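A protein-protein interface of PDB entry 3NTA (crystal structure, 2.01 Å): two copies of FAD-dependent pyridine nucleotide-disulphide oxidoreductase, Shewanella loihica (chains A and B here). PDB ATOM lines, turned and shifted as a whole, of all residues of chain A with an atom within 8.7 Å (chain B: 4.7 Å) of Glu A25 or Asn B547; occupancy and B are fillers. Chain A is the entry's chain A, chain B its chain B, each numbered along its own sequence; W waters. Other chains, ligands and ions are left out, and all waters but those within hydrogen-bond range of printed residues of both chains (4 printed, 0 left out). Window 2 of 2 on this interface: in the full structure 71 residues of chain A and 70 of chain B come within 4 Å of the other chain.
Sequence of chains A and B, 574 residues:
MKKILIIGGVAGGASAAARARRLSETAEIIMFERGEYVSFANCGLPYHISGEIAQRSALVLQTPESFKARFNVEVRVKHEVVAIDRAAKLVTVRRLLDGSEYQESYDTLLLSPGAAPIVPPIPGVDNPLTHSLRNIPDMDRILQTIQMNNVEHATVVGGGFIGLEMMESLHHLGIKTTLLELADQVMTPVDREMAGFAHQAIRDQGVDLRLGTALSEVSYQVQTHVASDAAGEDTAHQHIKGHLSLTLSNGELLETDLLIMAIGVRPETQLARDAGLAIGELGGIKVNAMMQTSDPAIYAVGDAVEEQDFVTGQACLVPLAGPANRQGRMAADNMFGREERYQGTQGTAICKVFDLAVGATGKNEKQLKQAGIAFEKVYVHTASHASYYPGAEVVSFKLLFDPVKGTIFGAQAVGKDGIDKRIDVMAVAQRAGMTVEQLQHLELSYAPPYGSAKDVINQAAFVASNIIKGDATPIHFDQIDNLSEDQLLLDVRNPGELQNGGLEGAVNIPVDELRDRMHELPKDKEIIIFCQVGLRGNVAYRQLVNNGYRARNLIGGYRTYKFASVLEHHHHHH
The backbone carbonyl oxygen of Arg A22 is in hydrogen-bond range of the side-chain amide nitrogen of Asn B546 (3.0 Å). The side-chain carboxylate (OE2) of Glu A25 lies within salt-bridge range of the guanidinium group (NH2) of Arg B515 (3.0 Å). O of Ala A69 is in hydrogen-bond range of NH1 of Arg B515. The backbone carbonyl oxygen of Arg A70 is in hydrogen-bond range of the guanidinium group of Arg B515, 2.9 Å away. O of Arg A70 sits at hydrogen-bond distance from NE2 of Gln B543, at 3.4 Å. The guanidinium group (NH1) of Arg B515 sits close to the backbone NH (N) of Asn A72.
The guanidinium group of Arg A21 sits at hydrogen-bond distance from the backbone carbonyl oxygen of Ser A24. The guanidinium group of Arg A21 sits at hydrogen-bond distance from the backbone carbonyl oxygen of Glu A25, at 3.4 Å. O of Phe A71 lies within hydrogen-bond range of NE of Arg A21. OG1 of Thr A26 is in hydrogen-bond range of OG of Ser A24, 3.3 Å away. The guanidinium group of Arg B515 sits close to the side-chain amide nitrogen of Gln B543 (3.4 Å). The side-chain amino group (NZ) of Lys B523 sits at hydrogen-bond distance from the backbone carbonyl oxygen (O) of Asn B547 (3.1 Å).
NH2 of Arg B515 touches CG of Arg A21, 3.8 Å away. Asn B546 touches Arg A21. C of Leu A23 touches ND2 of Asn B546 (3.8 Å). Ser A24 touches Asn B546 (N to ND2, 3.6 Å). OE2 of Glu A25 touches CG of Gln B543, at 3.0 Å. Glu A25 touches Asn B546 (CG to CB, 3.5 Å). Glu A25 touches Asn B547 (CG to ND2, 3.4 Å). Phe A71 touches Arg B515 (C to NH1, 3.8 Å).
Ala A20 touches none of the printed residues of chain B. Of the printed residues of chain B, Arg A21 touches Arg B515 and Asn B546. Of chain B, only Arg B515 (3.0 Å), Gln B543 (3.0 Å), Asn B546 (3.5 Å) and Asn B547 (3.4 Å) come within 4 Å of Glu A25. Ile A29 touches none of the printed residues of chain B. Of the printed residues of chain B, Ala A69 touches Arg B515 (3.3 Å). Asn B547 touches just one residue of chain A: Glu A25. Gly B548 touches none of the printed residues of chain A. The nearest printed residue of chain B that does not touch Glu A25 is Leu B544 (5.7 Å). The nearest printed residue of chain B that does not touch Arg A22 is Gln B543 (5.8 Å).
Of the 19 printed residues of chain A, 9 touch a printed residue of chain B. Of the 10 printed residues of chain B, 4 touch a printed residue of chain A. Printed residues of chain B that touch a printed residue of chain A: Arg B515, Gln B543, Asn B546 and Asn B547. Among the printed residues, Asp or Glu carboxylates within 4 Å of a Lys or Arg side-chain nitrogen of the other chain: Glu A25 with Arg B515 (3.0 Å).
No position is printed for both chains.
Water W3 lies within hydrogen-bond range of the backbone carbonyl oxygen of Arg A70 (2.7 Å), the side-chain amide nitrogen of Gln B543 (3.0 Å) and the guanidinium group of Arg B515 (3.0 Å). Water W2 lies within hydrogen-bond range of OE2 of Glu A25, O of Arg A21 and ND2 of Asn B546. Water W1 lies within hydrogen-bond range of the backbone NH (N) of Arg B515 (3.0 Å), the backbone carbonyl oxygen (O) of Ala A69 (3.0 Å) and the side-chain amide nitrogen (NE2) of Gln B543 (3.4 Å). Water W4 lies within hydrogen-bond range of O of Ala A69 (3.0 Å) and NH1 of Arg B515 (3.1 Å).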
ATOM      1  N   MET A   1     -10.847   3.094  16.718  1.00  0.00           N
ATOM      2  CA  MET A   1     -12.003   2.797  17.644  1.00  0.00           C
ATOM      3  C   MET A   1     -12.339   4.154  18.253  1.00  0.00           C
ATOM      4  O   MET A   1     -11.424   4.931  18.523  1.00  0.00           O
ATOM      5  CB  MET A   1     -11.560   1.896  18.749  1.00  0.00           C
ATOM      6  CG  MET A   1     -10.520   2.620  19.550  1.00  0.00           C
ATOM      7  SD  MET A   1     -10.101   1.906  21.282  1.00  0.00           S
ATOM      8  CE  MET A   1     -11.736   2.107  22.234  1.00  0.00           C
ATOM      9  N   LYS A   2     -13.610   4.485  18.393  1.00  0.00           N
ATOM     10  CA  LYS A   2     -14.002   5.876  18.836  1.00  0.00           C
ATOM     11  C   LYS A   2     -14.093   5.772  20.371  1.00  0.00           C
ATOM     12  O   LYS A   2     -14.642   4.824  20.858  1.00  0.00           O
ATOM     13  CB  LYS A   2     -15.366   6.271  18.345  1.00  0.00           C
ATOM     14  CG  LYS A   2     -15.648   6.194  16.840  1.00  0.00           C
ATOM     15  CD  LYS A   2     -17.020   6.856  16.524  1.00  0.00           C
ATOM     16  CE  LYS A   2     -16.864   7.973  15.510  1.00  0.00           C
ATOM     17  NZ  LYS A   2     -16.977   7.467  14.140  1.00  0.00           N
ATOM     18  N   ARG A  19     -27.850   2.095  22.396  1.00  0.00           N
ATOM     19  CA  ARG A  19     -27.730   2.220  20.901  1.00  0.00           C
ATOM     20  C   ARG A  19     -26.304   2.194  20.274  1.00  0.00           C
ATOM     21  O   ARG A  19     -26.099   1.574  19.128  1.00  0.00           O
ATOM     22  CB  ARG A  19     -28.567   3.378  20.319  1.00  0.00           C
ATOM     23  CG  ARG A  19     -28.373   3.480  18.769  1.00  0.00           C
ATOM     24  CD  ARG A  19     -29.187   2.472  17.970  1.00  0.00           C
ATOM     25  NE  ARG A  19     -29.221   2.917  16.570  1.00  0.00           N
ATOM     26  CZ  ARG A  19     -29.562   2.196  15.523  1.00  0.00           C
ATOM     27  NH1 ARG A  19     -29.941   0.934  15.655  1.00  0.00           N
ATOM     28  NH2 ARG A  19     -29.614   2.740  14.301  1.00  0.00           N
ATOM     29  N   ALA A  20     -25.354   2.894  20.935  1.00  0.00           N
ATOM     30  CA  ALA A  20     -24.032   3.113  20.368  1.00  0.00           C
ATOM     31  C   ALA A  20     -23.349   1.709  20.417  1.00  0.00           C
ATOM     32  O   ALA A  20     -22.529   1.442  19.611  1.00  0.00           O
ATOM     33  CB  ALA A  20     -23.160   4.150  21.237  1.00  0.00           C
ATOM     34  N   ARG A  21     -23.668   0.877  21.395  1.00  0.00           N
ATOM     35  CA  ARG A  21     -23.033  -0.486  21.507  1.00  0.00           C
ATOM     36  C   ARG A  21     -23.552  -1.377  20.454  1.00  0.00           C
ATOM     37  O   ARG A  21     -22.769  -2.169  19.893  1.00  0.00           O
ATOM     38  CB  ARG A  21     -23.171  -1.151  22.905  1.00  0.00           C
ATOM     39  CG  ARG A  21     -22.566  -2.665  22.938  1.00  0.00           C
ATOM     40  CD  ARG A  21     -21.008  -2.660  22.595  1.00  0.00           C
ATOM     41  NE  ARG A  21     -20.157  -1.959  23.577  1.00  0.00           N
ATOM     42  CZ  ARG A  21     -19.038  -1.240  23.340  1.00  0.00           C
ATOM     43  NH1 ARG A  21     -18.599  -0.912  22.099  1.00  0.00           N
ATOM     44  NH2 ARG A  21     -18.342  -0.804  24.409  1.00  0.00           N
ATOM     45  N   ARG A  22     -24.844  -1.282  20.138  1.00  0.00           N
ATOM     46  CA  ARG A  22     -25.418  -2.113  19.042  1.00  0.00           C
ATOM     47  C   ARG A  22     -24.850  -1.749  17.733  1.00  0.00           C
ATOM     48  O   ARG A  22     -24.621  -2.640  16.877  1.00  0.00           O
ATOM     49  CB  ARG A  22     -26.953  -2.131  19.012  1.00  0.00           C
ATOM     50  CG  ARG A  22     -27.673  -2.650  20.335  1.00  0.00           C
ATOM     51  CD  ARG A  22     -29.281  -2.662  20.150  1.00  0.00           C
ATOM     52  NE  ARG A  22     -29.945  -1.322  20.203  1.00  0.00           N
ATOM     53  CZ  ARG A  22     -30.389  -0.779  21.342  1.00  0.00           C
ATOM     54  NH1 ARG A  22     -30.170  -1.460  22.478  1.00  0.00           N
ATOM     55  NH2 ARG A  22     -31.056   0.454  21.375  1.00  0.00           N
ATOM     56  N   LEU A  23     -24.556  -0.475  17.519  1.00  0.00           N
ATOM     57  CA  LEU A  23     -23.836  -0.050  16.345  1.00  0.00           C
ATOM     58  C   LEU A  23     -22.384  -0.486  16.179  1.00  0.00           C
ATOM     59  O   LEU A  23     -21.926  -0.421  15.047  1.00  0.00           O
ATOM     60  CB  LEU A  23     -23.805   1.491  16.209  1.00  0.00           C
ATOM     61  CG  LEU A  23     -25.214   2.041  16.044  1.00  0.00           C
ATOM     62  CD1 LEU A  23     -25.241   3.643  16.236  1.00  0.00           C
ATOM     63  CD2 LEU A  23     -25.936   1.484  14.793  1.00  0.00           C
ATOM     64  N   SER A  24     -21.602  -0.692  17.258  1.00  0.00           N
ATOM     65  CA  SER A  24     -20.125  -0.972  17.092  1.00  0.00           C
ATOM     66  C   SER A  24     -19.600  -1.721  18.310  1.00  0.00           C
ATOM     67  O   SER A  24     -19.808  -1.216  19.441  1.00  0.00           O
ATOM     68  CB  SER A  24     -19.299   0.308  16.857  1.00  0.00           C
ATOM     69  OG  SER A  24     -17.971   0.172  17.394  1.00  0.00           O
ATOM     70  N   GLU A  25     -18.931  -2.896  18.124  1.00  0.00           N
ATOM     71  CA  GLU A  25     -18.324  -3.635  19.279  1.00  0.00           C
ATOM     72  C   GLU A  25     -16.961  -3.120  19.686  1.00  0.00           C
ATOM     73  O   GLU A  25     -16.544  -3.310  20.835  1.00  0.00           O
ATOM     74  CB  GLU A  25     -18.132  -5.157  19.007  1.00  0.00           C
ATOM     75  CG  GLU A  25     -19.425  -6.026  19.290  1.00  0.00           C
ATOM     76  CD  GLU A  25     -19.863  -6.146  20.746  1.00  0.00           C
ATOM     77  OE1 GLU A  25     -18.964  -6.036  21.611  1.00  0.00           O
ATOM     78  OE2 GLU A  25     -21.065  -6.441  20.957  1.00  0.00           O
ATOM     79  N   THR A  26     -16.273  -2.501  18.729  1.00  0.00           N
ATOM     80  CA  THR A  26     -14.952  -1.861  18.975  1.00  0.00           C
ATOM     81  C   THR A  26     -14.924  -0.534  19.831  1.00  0.00           C
ATOM     82  O   THR A  26     -13.952  -0.311  20.596  1.00  0.00           O
ATOM     83  CB  THR A  26     -14.182  -1.648  17.648  1.00  0.00           C
ATOM     84  OG1 THR A  26     -14.833  -0.655  16.799  1.00  0.00           O
ATOM     85  CG2 THR A  26     -14.061  -3.022  16.825  1.00  0.00           C
ATOM     86  N   ALA A  27     -15.988   0.296  19.793  1.00  0.00           N
ATOM     87  CA  ALA A  27     -15.909   1.597  20.578  1.00  0.00           C
ATOM     88  C   ALA A  27     -15.757   1.523  22.079  1.00  0.00           C
ATOM     89  O   ALA A  27     -16.249   0.649  22.690  1.00  0.00           O
ATOM     90  CB  ALA A  27     -16.983   2.561  20.161  1.00  0.00           C
ATOM     91  N   GLU A  28     -15.019   2.449  22.678  1.00  0.00           N
ATOM     92  CA  GLU A  28     -15.006   2.586  24.121  1.00  0.00           C
ATOM     93  C   GLU A  28     -16.124   3.592  24.529  1.00  0.00           C
ATOM     94  O   GLU A  28     -16.124   4.726  24.072  1.00  0.00           O
ATOM     95  CB  GLU A  28     -13.641   3.111  24.650  1.00  0.00           C
ATOM     96  CG  GLU A  28     -13.514   2.886  26.169  1.00  0.00           C
ATOM     97  CD  GLU A  28     -12.094   3.193  26.789  1.00  0.00           C
ATOM     98  OE1 GLU A  28     -11.392   3.780  25.963  1.00  0.00           O
ATOM     99  OE2 GLU A  28     -11.733   2.873  27.953  1.00  0.00           O
ATOM    100  N   ILE A  29     -16.990   3.152  25.410  1.00  0.00           N
ATOM    101  CA  ILE A  29     -18.141   3.916  25.923  1.00  0.00           C
ATOM    102  C   ILE A  29     -18.105   4.046  27.428  1.00  0.00           C
ATOM    103  O   ILE A  29     -18.189   3.054  28.139  1.00  0.00           O
ATOM    104  CB  ILE A  29     -19.487   3.233  25.537  1.00  0.00           C
ATOM    105  CG1 ILE A  29     -19.556   3.006  23.962  1.00  0.00           C
ATOM    106  CG2 ILE A  29     -20.700   4.166  25.949  1.00  0.00           C
ATOM    107  CD1 ILE A  29     -20.763   2.143  23.411  1.00  0.00           C
ATOM    108  N   ALA A  69     -22.475  -6.093  31.667  1.00  0.00           N
ATOM    109  CA  ALA A  69     -22.656  -7.453  31.193  1.00  0.00           C
ATOM    110  C   ALA A  69     -23.313  -7.493  29.803  1.00  0.00           C
ATOM    111  O   ALA A  69     -22.805  -8.135  28.870  1.00  0.00           O
ATOM    112  CB  ALA A  69     -23.430  -8.243  32.215  1.00  0.00           C
ATOM    113  N   ARG A  70     -24.342  -6.654  29.600  1.00  0.00           N
ATOM    114  CA  ARG A  70     -25.111  -6.681  28.366  1.00  0.00           C
ATOM    115  C   ARG A  70     -24.424  -5.874  27.248  1.00  0.00           C
ATOM    116  O   ARG A  70     -24.313  -6.359  26.080  1.00  0.00           O
ATOM    117  CB  ARG A  70     -26.645  -6.303  28.572  1.00  0.00           C
ATOM    118  CG  ARG A  70     -27.366  -6.200  27.267  1.00  0.00           C
ATOM    119  CD  ARG A  70     -28.948  -6.401  27.367  1.00  0.00           C
ATOM    120  NE  ARG A  70     -29.326  -7.427  28.360  1.00  0.00           N
ATOM    121  CZ  ARG A  70     -30.580  -7.790  28.652  1.00  0.00           C
ATOM    122  NH1 ARG A  70     -31.591  -7.114  28.122  1.00  0.00           N
ATOM    123  NH2 ARG A  70     -30.838  -8.805  29.487  1.00  0.00           N
ATOM    124  N   PHE A  71     -23.989  -4.664  27.577  1.00  0.00           N
ATOM    125  CA  PHE A  71     -23.526  -3.721  26.620  1.00  0.00           C
ATOM    126  C   PHE A  71     -22.079  -3.349  26.789  1.00  0.00           C
ATOM    127  O   PHE A  71     -21.622  -2.397  26.130  1.00  0.00           O
ATOM    128  CB  PHE A  71     -24.433  -2.418  26.722  1.00  0.00           C
ATOM    129  CG  PHE A  71     -25.869  -2.653  26.184  1.00  0.00           C
ATOM    130  CD1 PHE A  71     -26.117  -2.921  24.834  1.00  0.00           C
ATOM    131  CD2 PHE A  71     -26.918  -2.662  27.037  1.00  0.00           C
ATOM    132  CE1 PHE A  71     -27.451  -3.179  24.385  1.00  0.00           C
ATOM    133  CE2 PHE A  71     -28.246  -2.934  26.585  1.00  0.00           C
ATOM    134  CZ  PHE A  71     -28.492  -3.163  25.303  1.00  0.00           C
ATOM    135  N   ASN A  72     -21.360  -3.970  27.717  1.00  0.00           N
ATOM    136  CA  ASN A  72     -19.948  -3.625  27.952  1.00  0.00           C
ATOM    137  C   ASN A  72     -19.602  -2.145  28.252  1.00  0.00           C
ATOM    138  O   ASN A  72     -18.428  -1.775  28.273  1.00  0.00           O
ATOM    139  CB  ASN A  72     -19.083  -4.129  26.793  1.00  0.00           C
ATOM    140  CG  ASN A  72     -17.600  -4.073  27.104  1.00  0.00           C
ATOM    141  OD1 ASN A  72     -17.193  -4.175  28.262  1.00  0.00           O
ATOM    142  ND2 ASN A  72     -16.784  -3.911  26.070  1.00  0.00           N
ATOM    143  N   VAL A  73     -20.617  -1.314  28.483  1.00  0.00           N
ATOM    144  CA  VAL A  73     -20.449   0.138  28.841  1.00  0.00           C
ATOM    145  C   VAL A  73     -20.018   0.316  30.292  1.00  0.00           C
ATOM    146  O   VAL A  73     -20.599  -0.265  31.190  1.00  0.00           O
ATOM    147  CB  VAL A  73     -21.815   0.925  28.696  1.00  0.00           C
ATOM    148  CG1 VAL A  73     -21.687   2.447  29.150  1.00  0.00           C
ATOM    149  CG2 VAL A  73     -22.387   0.710  27.235  1.00  0.00           C
ATOM    150  N   PHE A 336     -21.854   7.896  14.925  1.00  0.00           N
ATOM    151  CA  PHE A 336     -21.170   7.039  13.970  1.00  0.00           C
ATOM    152  C   PHE A 336     -21.390   7.502  12.555  1.00  0.00           C
ATOM    153  O   PHE A 336     -21.370   6.693  11.630  1.00  0.00           O
ATOM    154  CB  PHE A 336     -21.577   5.582  14.201  1.00  0.00           C
ATOM    155  CG  PHE A 336     -21.118   5.080  15.493  1.00  0.00           C
ATOM    156  CD1 PHE A 336     -19.857   4.446  15.582  1.00  0.00           C
ATOM    157  CD2 PHE A 336     -21.844   5.303  16.629  1.00  0.00           C
ATOM    158  CE1 PHE A 336     -19.363   3.987  16.813  1.00  0.00           C
ATOM    159  CE2 PHE A 336     -21.418   4.841  17.855  1.00  0.00           C
ATOM    160  CZ  PHE A 336     -20.108   4.175  17.949  1.00  0.00           C
ATOM    161  N   ARG B 515     -20.963 -12.077  25.348  1.00  0.00           N
ATOM    162  CA  ARG B 515     -19.758 -11.397  24.844  1.00  0.00           C
ATOM    163  C   ARG B 515     -18.512 -12.208  25.218  1.00  0.00           C
ATOM    164  O   ARG B 515     -17.653 -12.459  24.343  1.00  0.00           O
ATOM    165  CB  ARG B 515     -19.691  -9.915  25.217  1.00  0.00           C
ATOM    166  CG  ARG B 515     -18.355  -9.197  25.017  1.00  0.00           C
ATOM    167  CD  ARG B 515     -18.621  -7.680  25.474  1.00  0.00           C
ATOM    168  NE  ARG B 515     -19.639  -7.033  24.576  1.00  0.00           N
ATOM    169  CZ  ARG B 515     -20.919  -6.803  24.836  1.00  0.00           C
ATOM    170  NH1 ARG B 515     -21.450  -6.986  26.039  1.00  0.00           N
ATOM    171  NH2 ARG B 515     -21.645  -6.250  23.894  1.00  0.00           N
ATOM    172  N   MET B 518     -18.183 -16.242  23.559  1.00  0.00           N
ATOM    173  CA  MET B 518     -18.523 -16.253  22.145  1.00  0.00           C
ATOM    174  C   MET B 518     -17.603 -17.103  21.252  1.00  0.00           C
ATOM    175  O   MET B 518     -17.952 -17.395  20.155  1.00  0.00           O
ATOM    176  CB  MET B 518     -18.431 -14.846  21.623  1.00  0.00           C
ATOM    177  CG  MET B 518     -19.015 -14.648  20.233  1.00  0.00           C
ATOM    178  SD  MET B 518     -18.793 -12.688  19.884  1.00  0.00           S
ATOM    179  CE  MET B 518     -18.973 -12.572  18.153  1.00  0.00           C
ATOM    180  N   LYS B 523     -17.273 -19.733  13.713  1.00  0.00           N
ATOM    181  CA  LYS B 523     -17.517 -18.727  12.697  1.00  0.00           C
ATOM    182  C   LYS B 523     -17.983 -19.261  11.324  1.00  0.00           C
ATOM    183  O   LYS B 523     -18.559 -18.510  10.510  1.00  0.00           O
ATOM    184  CB  LYS B 523     -16.276 -17.844  12.555  1.00  0.00           C
ATOM    185  CG  LYS B 523     -16.469 -16.584  11.691  1.00  0.00           C
ATOM    186  CD  LYS B 523     -16.512 -15.374  12.592  1.00  0.00           C
ATOM    187  CE  LYS B 523     -15.139 -15.109  13.085  1.00  0.00           C
ATOM    188  NZ  LYS B 523     -14.968 -13.995  14.045  1.00  0.00           N
ATOM    189  N   GLN B 543     -24.254  -8.170  18.533  1.00  0.00           N
ATOM    190  CA  GLN B 543     -22.905  -8.605  18.944  1.00  0.00           C
ATOM    191  C   GLN B 543     -22.128  -9.569  17.960  1.00  0.00           C
ATOM    192  O   GLN B 543     -20.910  -9.452  17.761  1.00  0.00           O
ATOM    193  CB  GLN B 543     -22.978  -9.335  20.261  1.00  0.00           C
ATOM    194  CG  GLN B 543     -23.267  -8.397  21.485  1.00  0.00           C
ATOM    195  CD  GLN B 543     -23.072  -9.165  22.702  1.00  0.00           C
ATOM    196  OE1 GLN B 543     -22.224 -10.107  22.740  1.00  0.00           O
ATOM    197  NE2 GLN B 543     -23.822  -8.833  23.730  1.00  0.00           N
ATOM    198  N   LEU B 544     -22.845 -10.461  17.326  1.00  0.00           N
ATOM    199  CA  LEU B 544     -22.202 -11.460  16.451  1.00  0.00           C
ATOM    200  C   LEU B 544     -21.914 -10.909  15.121  1.00  0.00           C
ATOM    201  O   LEU B 544     -20.854 -11.098  14.592  1.00  0.00           O
ATOM    202  CB  LEU B 544     -23.079 -12.705  16.339  1.00  0.00           C
ATOM    203  CG  LEU B 544     -23.266 -13.381  17.677  1.00  0.00           C
ATOM    204  CD1 LEU B 544     -24.530 -14.159  17.770  1.00  0.00           C
ATOM    205  CD2 LEU B 544     -22.099 -14.332  18.047  1.00  0.00           C
ATOM    206  N   VAL B 545     -22.865 -10.157  14.578  1.00  0.00           N
ATOM    207  CA  VAL B 545     -22.670  -9.490  13.296  1.00  0.00           C
ATOM    208  C   VAL B 545     -21.553  -8.446  13.364  1.00  0.00           C
ATOM    209  O   VAL B 545     -20.903  -8.158  12.359  1.00  0.00           O
ATOM    210  CB  VAL B 545     -23.965  -8.809  12.812  1.00  0.00           C
ATOM    211  CG1 VAL B 545     -23.773  -7.303  12.730  1.00  0.00           C
ATOM    212  CG2 VAL B 545     -24.390  -9.374  11.466  1.00  0.00           C
ATOM    213  N   ASN B 546     -21.335  -7.884  14.549  1.00  0.00           N
ATOM    214  CA  ASN B 546     -20.328  -6.888  14.737  1.00  0.00           C
ATOM    215  C   ASN B 546     -18.959  -7.553  14.906  1.00  0.00           C
ATOM    216  O   ASN B 546     -17.964  -6.922  14.664  1.00  0.00           O
ATOM    217  CB  ASN B 546     -20.594  -6.000  15.979  1.00  0.00           C
ATOM    218  CG  ASN B 546     -21.482  -4.842  15.696  1.00  0.00           C
ATOM    219  OD1 ASN B 546     -21.716  -4.524  14.537  1.00  0.00           O
ATOM    220  ND2 ASN B 546     -22.112  -4.261  16.758  1.00  0.00           N
ATOM    221  N   ASN B 547     -18.922  -8.816  15.253  1.00  0.00           N
ATOM    222  CA  ASN B 547     -17.676  -9.590  15.190  1.00  0.00           C
ATOM    223  C   ASN B 547     -17.416 -10.513  13.966  1.00  0.00           C
ATOM    224  O   ASN B 547     -16.561 -11.384  14.054  1.00  0.00           O
ATOM    225  CB  ASN B 547     -17.631 -10.434  16.424  1.00  0.00           C
ATOM    226  CG  ASN B 547     -17.260  -9.633  17.643  1.00  0.00           C
ATOM    227  OD1 ASN B 547     -16.093  -9.478  17.903  1.00  0.00           O
ATOM    228  ND2 ASN B 547     -18.261  -9.090  18.387  1.00  0.00           N
ATOM    229  N   GLY B 548     -18.169 -10.344  12.881  1.00  0.00           N
ATOM    230  CA  GLY B 548     -17.977 -11.046  11.581  1.00  0.00           C
ATOM    231  C   GLY B 548     -18.685 -12.398  11.384  1.00  0.00           C
ATOM    232  O   GLY B 548     -18.358 -13.202  10.479  1.00  0.00           O
ATOM    233  N   TYR B 549     -19.646 -12.698  12.240  1.00  0.00           N
ATOM    234  CA  TYR B 549     -20.467 -13.861  12.040  1.00  0.00           C
ATOM    235  C   TYR B 549     -21.616 -13.545  11.105  1.00  0.00           C
ATOM    236  O   TYR B 549     -22.045 -12.340  10.963  1.00  0.00           O
ATOM    237  CB  TYR B 549     -21.058 -14.302  13.345  1.00  0.00           C
ATOM    238  CG  TYR B 549     -20.138 -14.959  14.356  1.00  0.00           C
ATOM    239  CD1 TYR B 549     -19.248 -14.208  15.121  1.00  0.00           C
ATOM    240  CD2 TYR B 549     -20.222 -16.344  14.600  1.00  0.00           C
ATOM    241  CE1 TYR B 549     -18.454 -14.835  16.131  1.00  0.00           C
ATOM    242  CE2 TYR B 549     -19.452 -16.972  15.573  1.00  0.00           C
ATOM    243  CZ  TYR B 549     -18.574 -16.219  16.315  1.00  0.00           C
ATOM    244  OH  TYR B 549     -17.836 -16.841  17.256  1.00  0.00           O
HETATM  245  O   HOH W   1     -22.828 -10.205  26.670  1.00  0.00           O
HETATM  246  O   HOH W   2     -22.997  -4.961  19.574  1.00  0.00           O
HETATM  247  O   HOH W   3     -24.626  -5.999  23.466  1.00  0.00           O
HETATM  248  O   HOH W   4     -19.878  -7.765  28.654  1.00  0.00           O
